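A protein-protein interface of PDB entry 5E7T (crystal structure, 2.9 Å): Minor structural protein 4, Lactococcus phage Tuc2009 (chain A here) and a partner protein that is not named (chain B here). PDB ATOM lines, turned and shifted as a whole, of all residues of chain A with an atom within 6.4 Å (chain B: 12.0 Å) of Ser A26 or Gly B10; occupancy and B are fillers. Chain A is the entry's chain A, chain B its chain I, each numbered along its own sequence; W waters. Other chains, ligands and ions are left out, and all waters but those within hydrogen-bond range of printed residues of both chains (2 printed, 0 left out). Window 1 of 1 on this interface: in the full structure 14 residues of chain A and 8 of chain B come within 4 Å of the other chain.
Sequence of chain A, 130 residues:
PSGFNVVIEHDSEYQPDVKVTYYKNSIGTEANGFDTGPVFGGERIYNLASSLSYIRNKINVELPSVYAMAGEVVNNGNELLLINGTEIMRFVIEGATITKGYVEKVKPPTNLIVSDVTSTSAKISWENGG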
ATOM      1  N   TYR A  23      20.624  28.437 -13.119  1.00  0.00           N
ATOM      2  CA  TYR A  23      19.447  28.101 -13.916  1.00  0.00           C
ATOM      3  C   TYR A  23      18.570  29.317 -14.192  1.00  0.00           C
ATOM      4  O   TYR A  23      18.492  30.243 -13.370  1.00  0.00           O
ATOM      5  CB  TYR A  23      18.636  26.960 -13.290  1.00  0.00           C
ATOM      6  CG  TYR A  23      18.286  27.165 -11.835  1.00  0.00           C
ATOM      7  CD1 TYR A  23      19.120  26.700 -10.826  1.00  0.00           C
ATOM      8  CD2 TYR A  23      17.108  27.803 -11.467  1.00  0.00           C
ATOM      9  CE1 TYR A  23      18.814  26.908  -9.485  1.00  0.00           C
ATOM     10  CE2 TYR A  23      16.791  28.015 -10.126  1.00  0.00           C
ATOM     11  CZ  TYR A  23      17.635  27.542  -9.138  1.00  0.00           C
ATOM     12  OH  TYR A  23      17.302  27.719  -7.819  1.00  0.00           O
ATOM     13  N   LYS A  24      17.934  29.311 -15.373  1.00  0.00           N
ATOM     14  CA  LYS A  24      17.056  30.361 -15.860  1.00  0.00           C
ATOM     15  C   LYS A  24      15.602  29.920 -15.811  1.00  0.00           C
ATOM     16  O   LYS A  24      15.293  28.763 -16.105  1.00  0.00           O
ATOM     17  CB  LYS A  24      17.394  30.631 -17.325  1.00  0.00           C
ATOM     18  CG  LYS A  24      18.303  31.801 -17.543  1.00  0.00           C
ATOM     19  CD  LYS A  24      18.990  31.756 -18.888  1.00  0.00           C
ATOM     20  CE  LYS A  24      18.141  32.090 -20.079  1.00  0.00           C
ATOM     21  NZ  LYS A  24      18.910  32.886 -21.072  1.00  0.00           N
ATOM     22  N   ASN A  25      14.698  30.876 -15.552  1.00  0.00           N
ATOM     23  CA  ASN A  25      13.233  30.724 -15.611  1.00  0.00           C
ATOM     24  C   ASN A  25      12.620  29.663 -14.676  1.00  0.00           C
ATOM     25  O   ASN A  25      11.553  29.111 -14.989  1.00  0.00           O
ATOM     26  CB  ASN A  25      12.741  30.504 -17.054  1.00  0.00           C
ATOM     27  CG  ASN A  25      12.931  31.705 -17.928  1.00  0.00           C
ATOM     28  OD1 ASN A  25      12.363  32.772 -17.691  1.00  0.00           O
ATOM     29  ND2 ASN A  25      13.714  31.548 -18.971  1.00  0.00           N
ATOM     30  N   SER A  26      13.213  29.485 -13.478  1.00  0.00           N
ATOM     31  CA  SER A  26      12.640  28.670 -12.397  1.00  0.00           C
ATOM     32  C   SER A  26      11.315  29.382 -11.956  1.00  0.00           C
ATOM     33  O   SER A  26      11.103  30.533 -12.340  1.00  0.00           O
ATOM     34  CB  SER A  26      13.608  28.616 -11.225  1.00  0.00           C
ATOM     35  OG  SER A  26      14.106  29.910 -10.916  1.00  0.00           O
ATOM     36  N   ILE A  27      10.426  28.713 -11.193  1.00  0.00           N
ATOM     37  CA  ILE A  27       9.124  29.284 -10.808  1.00  0.00           C
ATOM     38  C   ILE A  27       9.278  30.609 -10.066  1.00  0.00           C
ATOM     39  O   ILE A  27       9.989  30.668  -9.075  1.00  0.00           O
ATOM     40  CB  ILE A  27       8.181  28.283 -10.061  1.00  0.00           C
ATOM     41  CG1 ILE A  27       8.843  27.604  -8.848  1.00  0.00           C
ATOM     42  CG2 ILE A  27       7.623  27.245 -11.044  1.00  0.00           C
ATOM     43  CD1 ILE A  27       7.964  27.468  -7.699  1.00  0.00           C
ATOM     44  N   GLY A  28       8.667  31.663 -10.597  1.00  0.00           N
ATOM     45  CA  GLY A  28       8.697  32.981  -9.967  1.00  0.00           C
ATOM     46  C   GLY A  28       9.667  33.992 -10.541  1.00  0.00           C
ATOM     47  O   GLY A  28       9.632  35.165 -10.139  1.00  0.00           O
ATOM     48  N   THR A  29      10.523  33.551 -11.497  1.00  0.00           N
ATOM     49  CA  THR A  29      11.518  34.380 -12.187  1.00  0.00           C
ATOM     50  C   THR A  29      11.191  34.670 -13.672  1.00  0.00           C
ATOM     51  O   THR A  29      11.877  35.474 -14.316  1.00  0.00           O
ATOM     52  CB  THR A  29      12.891  33.798 -12.044  1.00  0.00           C
ATOM     53  OG1 THR A  29      12.934  32.609 -12.814  1.00  0.00           O
ATOM     54  CG2 THR A  29      13.261  33.522 -10.605  1.00  0.00           C
ATOM     55  N   GLU A  30      10.130  34.045 -14.204  1.00  0.00           N
ATOM     56  CA  GLU A  30       9.688  34.252 -15.585  1.00  0.00           C
ATOM     57  C   GLU A  30       9.306  35.716 -15.762  1.00  0.00           C
ATOM     58  O   GLU A  30       8.702  36.308 -14.856  1.00  0.00           O
ATOM     59  CB  GLU A  30       8.512  33.335 -15.944  1.00  0.00           C
ATOM     60  CG  GLU A  30       8.716  31.874 -15.600  1.00  0.00           C
ATOM     61  CD  GLU A  30       8.058  31.430 -14.307  1.00  0.00           C
ATOM     62  OE1 GLU A  30       8.069  32.203 -13.318  1.00  0.00           O
ATOM     63  OE2 GLU A  30       7.537  30.292 -14.288  1.00  0.00           O
ATOM     64  N   VAL A  39      10.313  26.602 -20.392  1.00  0.00           N
ATOM     65  CA  VAL A  39      10.471  25.283 -19.767  1.00  0.00           C
ATOM     66  C   VAL A  39       9.976  25.425 -18.325  1.00  0.00           C
ATOM     67  O   VAL A  39      10.761  25.840 -17.444  1.00  0.00           O
ATOM     68  CB  VAL A  39      11.947  24.764 -19.821  1.00  0.00           C
ATOM     69  CG1 VAL A  39      12.053  23.340 -19.295  1.00  0.00           C
ATOM     70  CG2 VAL A  39      12.567  24.882 -21.221  1.00  0.00           C
ATOM     71  N   GLY A  41       9.280  25.320 -14.666  1.00  0.00           N
ATOM     72  CA  GLY A  41      10.043  24.760 -13.552  1.00  0.00           C
ATOM     73  C   GLY A  41      11.506  25.111 -13.612  1.00  0.00           C
ATOM     74  O   GLY A  41      12.196  25.032 -12.603  1.00  0.00           O
ATOM     75  N   GLY A  42      11.973  25.500 -14.795  1.00  0.00           N
ATOM     76  CA  GLY A  42      13.355  25.909 -14.983  1.00  0.00           C
ATOM     77  C   GLY A  42      14.049  25.230 -16.136  1.00  0.00           C
ATOM     78  O   GLY A  42      13.831  24.045 -16.379  1.00  0.00           O
ATOM     79  N   GLU A  43      14.907  25.979 -16.840  1.00  0.00           N
ATOM     80  CA  GLU A  43      15.680  25.499 -17.982  1.00  0.00           C
ATOM     81  C   GLU A  43      16.864  24.677 -17.450  1.00  0.00           C
ATOM     82  O   GLU A  43      16.836  24.260 -16.291  1.00  0.00           O
ATOM     83  CB  GLU A  43      16.172  26.687 -18.825  1.00  0.00           C
ATOM     84  CG  GLU A  43      15.131  27.336 -19.716  1.00  0.00           C
ATOM     85  CD  GLU A  43      15.668  28.508 -20.526  1.00  0.00           C
ATOM     86  OE1 GLU A  43      16.720  28.364 -21.193  1.00  0.00           O
ATOM     87  OE2 GLU A  43      15.023  29.581 -20.491  1.00  0.00           O
ATOM     88  N   GLU A  79      19.872  27.464   1.812  1.00  0.00           N
ATOM     89  CA  GLU A  79      20.393  27.884   0.527  1.00  0.00           C
ATOM     90  C   GLU A  79      20.345  29.400   0.411  1.00  0.00           C
ATOM     91  O   GLU A  79      19.489  30.041   1.018  1.00  0.00           O
ATOM     92  CB  GLU A  79      19.539  27.266  -0.607  1.00  0.00           C
ATOM     93  CG  GLU A  79      18.089  27.760  -0.615  1.00  0.00           C
ATOM     94  CD  GLU A  79      17.205  27.548  -1.828  1.00  0.00           C
ATOM     95  OE1 GLU A  79      16.209  28.297  -1.965  1.00  0.00           O
ATOM     96  OE2 GLU A  79      17.451  26.587  -2.591  1.00  0.00           O
ATOM     97  N   LEU A  81      20.198  32.480  -2.636  1.00  0.00           N
ATOM     98  CA  LEU A  81      19.833  32.677  -4.032  1.00  0.00           C
ATOM     99  C   LEU A  81      20.265  34.050  -4.493  1.00  0.00           C
ATOM    100  O   LEU A  81      19.982  35.043  -3.824  1.00  0.00           O
ATOM    101  CB  LEU A  81      18.311  32.532  -4.236  1.00  0.00           C
ATOM    102  CG  LEU A  81      17.651  31.201  -3.903  1.00  0.00           C
ATOM    103  CD1 LEU A  81      16.168  31.276  -4.166  1.00  0.00           C
ATOM    104  CD2 LEU A  81      18.190  30.103  -4.724  1.00  0.00           C
ATOM    105  N   ILE A  83      19.325  36.300  -7.309  1.00  0.00           N
ATOM    106  CA  ILE A  83      18.309  36.443  -8.353  1.00  0.00           C
ATOM    107  C   ILE A  83      18.518  37.695  -9.158  1.00  0.00           C
ATOM    108  O   ILE A  83      18.424  38.781  -8.590  1.00  0.00           O
ATOM    109  CB  ILE A  83      16.852  36.388  -7.792  1.00  0.00           C
ATOM    110  CG1 ILE A  83      16.703  35.371  -6.628  1.00  0.00           C
ATOM    111  CG2 ILE A  83      15.863  36.102  -8.922  1.00  0.00           C
ATOM    112  CD1 ILE A  83      15.303  35.250  -6.019  1.00  0.00           C
ATOM    113  N   THR A  86      15.581  36.774 -14.503  1.00  0.00           N
ATOM    114  CA  THR A  86      15.273  35.418 -14.963  1.00  0.00           C
ATOM    115  C   THR A  86      16.314  34.391 -14.480  1.00  0.00           C
ATOM    116  O   THR A  86      16.026  33.189 -14.444  1.00  0.00           O
ATOM    117  CB  THR A  86      15.253  35.536 -16.503  1.00  0.00           C
ATOM    118  OG1 THR A  86      14.012  35.095 -17.024  1.00  0.00           O
ATOM    119  CG2 THR A  86      16.417  34.863 -17.198  1.00  0.00           C
ATOM    120  N   GLU A  87      17.547  34.878 -14.165  1.00  0.00           N
ATOM    121  CA  GLU A  87      18.717  34.097 -13.783  1.00  0.00           C
ATOM    122  C   GLU A  87      18.807  33.912 -12.316  1.00  0.00           C
ATOM    123  O   GLU A  87      18.634  34.867 -11.567  1.00  0.00           O
ATOM    124  CB  GLU A  87      19.996  34.813 -14.209  1.00  0.00           C
ATOM    125  CG  GLU A  87      20.229  34.921 -15.693  1.00  0.00           C
ATOM    126  CD  GLU A  87      21.457  35.753 -15.979  1.00  0.00           C
ATOM    127  OE1 GLU A  87      21.331  36.997 -15.999  1.00  0.00           O
ATOM    128  OE2 GLU A  87      22.560  35.170 -16.087  1.00  0.00           O
ATOM    129  N   ILE A  88      19.166  32.699 -11.898  1.00  0.00           N
ATOM    130  CA  ILE A  88      19.400  32.360 -10.506  1.00  0.00           C
ATOM    131  C   ILE A  88      20.686  31.599 -10.352  1.00  0.00           C
ATOM    132  O   ILE A  88      20.975  30.683 -11.117  1.00  0.00           O
ATOM    133  CB  ILE A  88      18.202  31.658  -9.812  1.00  0.00           C
ATOM    134  CG1 ILE A  88      17.243  32.714  -9.317  1.00  0.00           C
ATOM    135  CG2 ILE A  88      18.660  30.808  -8.617  1.00  0.00           C
ATOM    136  CD1 ILE A  88      16.151  32.228  -8.724  1.00  0.00           C
ATOM    137  N   ARG A  90      22.322  29.558  -7.333  1.00  0.00           N
ATOM    138  CA  ARG A  90      21.927  28.911  -6.099  1.00  0.00           C
ATOM    139  C   ARG A  90      23.163  28.357  -5.380  1.00  0.00           C
ATOM    140  O   ARG A  90      23.988  27.694  -6.012  1.00  0.00           O
ATOM    141  CB  ARG A  90      20.939  27.793  -6.454  1.00  0.00           C
ATOM    142  CG  ARG A  90      20.228  27.215  -5.265  1.00  0.00           C
ATOM    143  CD  ARG A  90      19.757  25.804  -5.518  1.00  0.00           C
ATOM    144  NE  ARG A  90      19.075  25.308  -4.332  1.00  0.00           N
ATOM    145  CZ  ARG A  90      18.776  24.040  -4.093  1.00  0.00           C
ATOM    146  NH1 ARG A  90      19.124  23.100  -4.950  1.00  0.00           N
ATOM    147  NH2 ARG A  90      18.161  23.698  -2.967  1.00  0.00           N
ATOM    148  N   THR B   5       6.975  20.312   1.753  1.00  0.00           N
ATOM    149  CA  THR B   5       8.204  21.075   1.522  1.00  0.00           C
ATOM    150  C   THR B   5       7.819  22.405   0.865  1.00  0.00           C
ATOM    151  O   THR B   5       7.095  22.425  -0.121  1.00  0.00           O
ATOM    152  CB  THR B   5       9.336  20.251   0.838  1.00  0.00           C
ATOM    153  OG1 THR B   5      10.106  21.090  -0.033  1.00  0.00           O
ATOM    154  CG2 THR B   5       8.847  18.980   0.134  1.00  0.00           C
ATOM    155  N   LYS B   6       8.272  23.517   1.474  1.00  0.00           N
ATOM    156  CA  LYS B   6       7.954  24.886   1.073  1.00  0.00           C
ATOM    157  C   LYS B   6       8.247  25.166  -0.380  1.00  0.00           C
ATOM    158  O   LYS B   6       9.327  24.819  -0.851  1.00  0.00           O
ATOM    159  CB  LYS B   6       8.664  25.900   1.996  1.00  0.00           C
ATOM    160  CG  LYS B   6       8.049  27.298   1.974  1.00  0.00           C
ATOM    161  CD  LYS B   6       8.878  28.288   2.782  1.00  0.00           C
ATOM    162  CE  LYS B   6       8.435  29.721   2.603  1.00  0.00           C
ATOM    163  NZ  LYS B   6       8.472  30.493   3.867  1.00  0.00           N
ATOM    164  N   ILE B   7       7.277  25.793  -1.076  1.00  0.00           N
ATOM    165  CA  ILE B   7       7.355  26.248  -2.468  1.00  0.00           C
ATOM    166  C   ILE B   7       7.731  27.735  -2.418  1.00  0.00           C
ATOM    167  O   ILE B   7       6.949  28.558  -1.915  1.00  0.00           O
ATOM    168  CB  ILE B   7       6.018  26.004  -3.227  1.00  0.00           C
ATOM    169  CG1 ILE B   7       5.586  24.522  -3.200  1.00  0.00           C
ATOM    170  CG2 ILE B   7       6.053  26.557  -4.646  1.00  0.00           C
ATOM    171  CD1 ILE B   7       6.597  23.541  -3.641  1.00  0.00           C
ATOM    172  N   THR B   8       8.946  28.061  -2.881  1.00  0.00           N
ATOM    173  CA  THR B   8       9.473  29.418  -2.849  1.00  0.00           C
ATOM    174  C   THR B   8       9.845  29.934  -4.244  1.00  0.00           C
ATOM    175  O   THR B   8      10.157  29.145  -5.135  1.00  0.00           O
ATOM    176  CB  THR B   8      10.709  29.494  -1.907  1.00  0.00           C
ATOM    177  OG1 THR B   8      11.764  28.663  -2.394  1.00  0.00           O
ATOM    178  CG2 THR B   8      10.395  29.135  -0.486  1.00  0.00           C
ATOM    179  N   ARG B   9       9.858  31.269  -4.406  1.00  0.00           N
ATOM    180  CA  ARG B   9      10.301  31.956  -5.607  1.00  0.00           C
ATOM    181  C   ARG B   9      11.762  31.615  -5.841  1.00  0.00           C
ATOM    182  O   ARG B   9      12.586  31.716  -4.911  1.00  0.00           O
ATOM    183  CB  ARG B   9      10.162  33.474  -5.407  1.00  0.00           C
ATOM    184  CG  ARG B   9      10.665  34.349  -6.562  1.00  0.00           C
ATOM    185  CD  ARG B   9      10.276  35.798  -6.347  1.00  0.00           C
ATOM    186  NE  ARG B   9      11.028  36.389  -5.242  1.00  0.00           N
ATOM    187  CZ  ARG B   9      12.111  37.138  -5.400  1.00  0.00           C
ATOM    188  NH1 ARG B   9      12.570  37.411  -6.622  1.00  0.00           N
ATOM    189  NH2 ARG B   9      12.740  37.633  -4.341  1.00  0.00           N
ATOM    190  N   GLY B  10      12.051  31.179  -7.061  1.00  0.00           N
ATOM    191  CA  GLY B  10      13.395  30.873  -7.523  1.00  0.00           C
ATOM    192  C   GLY B  10      13.960  29.532  -7.119  1.00  0.00           C
ATOM    193  O   GLY B  10      15.122  29.226  -7.443  1.00  0.00           O
ATOM    194  N   MET B  11      13.141  28.701  -6.437  1.00  0.00           N
ATOM    195  CA  MET B  11      13.571  27.371  -6.012  1.00  0.00           C
ATOM    196  C   MET B  11      13.960  26.538  -7.234  1.00  0.00           C
ATOM    197  O   MET B  11      13.388  26.724  -8.313  1.00  0.00           O
ATOM    198  CB  MET B  11      12.515  26.690  -5.122  1.00  0.00           C
ATOM    199  CG  MET B  11      11.349  26.099  -5.879  1.00  0.00           C
ATOM    200  SD  MET B  11      10.093  25.327  -4.833  1.00  0.00           S
ATOM    201  CE  MET B  11      11.003  24.092  -4.048  1.00  0.00           C
ATOM    202  N   GLN B  12      14.973  25.677  -7.080  1.00  0.00           N
ATOM    203  CA  GLN B  12      15.501  24.854  -8.153  1.00  0.00           C
ATOM    204  C   GLN B  12      14.522  23.796  -8.673  1.00  0.00           C
ATOM    205  O   GLN B  12      14.376  23.748  -9.886  1.00  0.00           O
ATOM    206  CB  GLN B  12      16.835  24.246  -7.732  1.00  0.00           C
ATOM    207  CG  GLN B  12      17.410  23.169  -8.628  1.00  0.00           C
ATOM    208  CD  GLN B  12      18.879  22.998  -8.400  1.00  0.00           C
ATOM    209  OE1 GLN B  12      19.614  23.964  -8.249  1.00  0.00           O
ATOM    210  NE2 GLN B  12      19.359  21.768  -8.404  1.00  0.00           N
ATOM    211  N   ASN B  13      13.886  22.941  -7.821  1.00  0.00           N
ATOM    212  CA  ASN B  13      12.981  21.884  -8.313  1.00  0.00           C
ATOM    213  C   ASN B  13      11.523  22.143  -7.943  1.00  0.00           C
ATOM    214  O   ASN B  13      10.875  21.355  -7.243  1.00  0.00           O
ATOM    215  CB  ASN B  13      13.452  20.500  -7.889  1.00  0.00           C
ATOM    216  CG  ASN B  13      14.847  20.183  -8.385  1.00  0.00           C
ATOM    217  OD1 ASN B  13      15.137  20.234  -9.587  1.00  0.00           O
ATOM    218  ND2 ASN B  13      15.748  19.860  -7.467  1.00  0.00           N
ATOM    219  N   GLY B  14      11.036  23.275  -8.444  1.00  0.00           N
ATOM    220  CA  GLY B  14       9.684  23.779  -8.228  1.00  0.00           C
ATOM    221  C   GLY B  14       8.608  22.843  -8.708  1.00  0.00           C
ATOM    222  O   GLY B  14       7.728  22.488  -7.935  1.00  0.00           O
ATOM    223  N   ALA B  15       8.702  22.394  -9.959  1.00  0.00           N
ATOM    224  CA  ALA B  15       7.761  21.471 -10.570  1.00  0.00           C
ATOM    225  C   ALA B  15       7.683  20.170  -9.796  1.00  0.00           C
ATOM    226  O   ALA B  15       6.577  19.719  -9.467  1.00  0.00           O
ATOM    227  CB  ALA B  15       8.167  21.197 -12.011  1.00  0.00           C
ATOM    228  N   GLU B  16       8.873  19.604  -9.461  1.00  0.00           N
ATOM    229  CA  GLU B  16       9.048  18.335  -8.736  1.00  0.00           C
ATOM    230  C   GLU B  16       8.529  18.411  -7.309  1.00  0.00           C
ATOM    231  O   GLU B  16       7.934  17.438  -6.840  1.00  0.00           O
ATOM    232  CB  GLU B  16      10.515  17.907  -8.737  1.00  0.00           C
ATOM    233  CG  GLU B  16      11.056  17.587 -10.109  1.00  0.00           C
ATOM    234  CD  GLU B  16      11.634  18.738 -10.900  1.00  0.00           C
ATOM    235  OE1 GLU B  16      11.492  19.899 -10.455  1.00  0.00           O
ATOM    236  OE2 GLU B  16      12.144  18.485 -12.016  1.00  0.00           O
ATOM    237  N   THR B  17       8.746  19.551  -6.625  1.00  0.00           N
ATOM    238  CA  THR B  17       8.296  19.728  -5.251  1.00  0.00           C
ATOM    239  C   THR B  17       6.785  19.949  -5.208  1.00  0.00           C
ATOM    240  O   THR B  17       6.134  19.412  -4.304  1.00  0.00           O
ATOM    241  CB  THR B  17       9.117  20.791  -4.523  1.00  0.00           C
ATOM    242  OG1 THR B  17      10.520  20.525  -4.676  1.00  0.00           O
ATOM    243  CG2 THR B  17       8.801  20.847  -3.066  1.00  0.00           C
ATOM    244  N   ILE B  18       6.216  20.685  -6.199  1.00  0.00           N
ATOM    245  CA  ILE B  18       4.765  20.901  -6.297  1.00  0.00           C
ATOM    246  C   ILE B  18       4.102  19.546  -6.483  1.00  0.00           C
ATOM    247  O   ILE B  18       3.155  19.231  -5.755  1.00  0.00           O
ATOM    248  CB  ILE B  18       4.374  21.916  -7.424  1.00  0.00           C
ATOM    249  CG1 ILE B  18       4.825  23.350  -7.054  1.00  0.00           C
ATOM    250  CG2 ILE B  18       2.866  21.878  -7.744  1.00  0.00           C
ATOM    251  CD1 ILE B  18       4.910  24.335  -8.192  1.00  0.00           C
HETATM  252  O   HOH W   1      11.078  22.752 -11.233  1.00  0.00           O
HETATM  253  O   HOH W   2      11.599  25.943 -10.177  1.00  0.00           O
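The side-chain hydroxyl (OH) of Tyr A23 sits at hydrogen-bond distance from the backbone NH (N) of Gln B12 (3.2 Å). O of Gly B10 is in hydrogen-bond range of OH of Tyr A23 (2.7 Å). NH1 of Arg A90 sits close to OE1 of Gln B12 (3.4 Å). The backbone carbonyl oxygen of Ile A27 sits at hydrogen-bond distance from the backbone NH of Gly B10, at 2.9 Å.
Among the printed residues, merely in contact across the chains: Ile A88 with Gly B10 (3.3 Å), Ser A26 with Met B11 (3.5 Å), Ile A83 with Arg B9 (3.5 Å), Tyr A23 with Met B11 (3.6 Å), Ser A26 with Gly B10 (3.6 Å), Leu A81 with Arg B9 (3.7 Å), Gly A41 with Gln B12 (3.7 Å), Ile A27 with Arg B9 (3.7 Å), Ile A27 with Ile B7 (3.7 Å), Ile A27 with Thr B8 (3.8 Å), Gly A28 with Arg B9 (3.8 Å) and Ile A27 with Gly B14 (3.97 Å).
O of Ser A26 is in hydrogen-bond range of OG1 of Thr A29 (2.8 Å). N of Gly A28 is in hydrogen-bond range of OE1 of Glu A30 (2.8 Å). The backbone carbonyl oxygen (O) of Tyr A23 sits at hydrogen-bond distance from the backbone NH (N) of Ile A88. OE2 of Glu A79 is in salt-bridge range of NE of Arg A90, at 2.7 Å. The side-chain sulfur of Met B11 sits at hydrogen-bond distance from the backbone NH of Thr B8, at 3.5 Å.
Tyr A23 touches just these residues of chain B: Gly B10 (2.7 Å), Met B11 (3.6 Å) and Gln B12 (3.2 Å). Asn A25 touches none of the printed residues of chain B. Of chain B, only Gly B10 (3.6 Å) and Met B11 (3.5 Å) come within 4 Å of Ser A26. Ile A27 touches five residues of chain B. Gly A28 touches just one residue of chain B: Arg B9 (3.8 Å). No residue of chain B comes within 4 Å of Glu A30. Gly A41 touches just one residue of chain B: Gln B12 (3.7 Å). Gly A42 touches none of the printed residues of chain B. Glu A43 touches none of the printed residues of chain B. Of the printed residues of chain B, Leu A81 touches Arg B9 (3.7 Å). No residue of chain B comes within 4 Å of Thr A86. Of the printed residues of chain B, Ile A88 touches Gly B10. Of the printed residues of chain A, Ile B7 touches Ile A27. Printed residues of chain A within 4 Å of Gly B10: Tyr A23 (2.7 Å), Ser A26 (3.6 Å), Ile A27 (2.9 Å) and Ile A88 (3.3 Å). Of the printed residues of chain A, Met B11 touches Tyr A23 (3.6 Å) and Ser A26 (3.5 Å). Glu B16 touches none of the printed residues of chain A. The nearest printed residue of chain A that does not touch Gly B10 is Leu A81 (4.004 Å). The nearest printed residue of chain B that does not touch Leu A81 is Gly B10 (4.004 Å).
Water W2 lies within hydrogen-bond range of the backbone carbonyl oxygen of Gly A41 (2.7 Å), the backbone carbonyl oxygen of Met B11 (2.7 Å), the backbone NH of Ile A27 (3.2 Å) and the backbone NH of Gly B14 (3.2 Å). Water W1 lies within hydrogen-bond range of N of Ala B15, N of Gly B14, O of Gly A41 and OE1 of Glu B16.
Hydrophobic or aromatic side chains of chain A that line the printed part of chain B: Tyr A23, Ile A27, Leu A81, Ile A83 and Ile A88. Along chain A the printed residues that touch a printed residue of chain B span positions 23 to 90. Printed residues of chain B that touch a printed residue of chain A: Ile B7, Thr B8, Arg B9, Gly B10, Met B11, Gln B12 and Gly B14. Among the printed residues, 16 pairs touch across the chains. Among the printed residues, no Asp or Glu carboxylate lies within 4 Å of a Lys or Arg side-chain nitrogen of the other chain.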
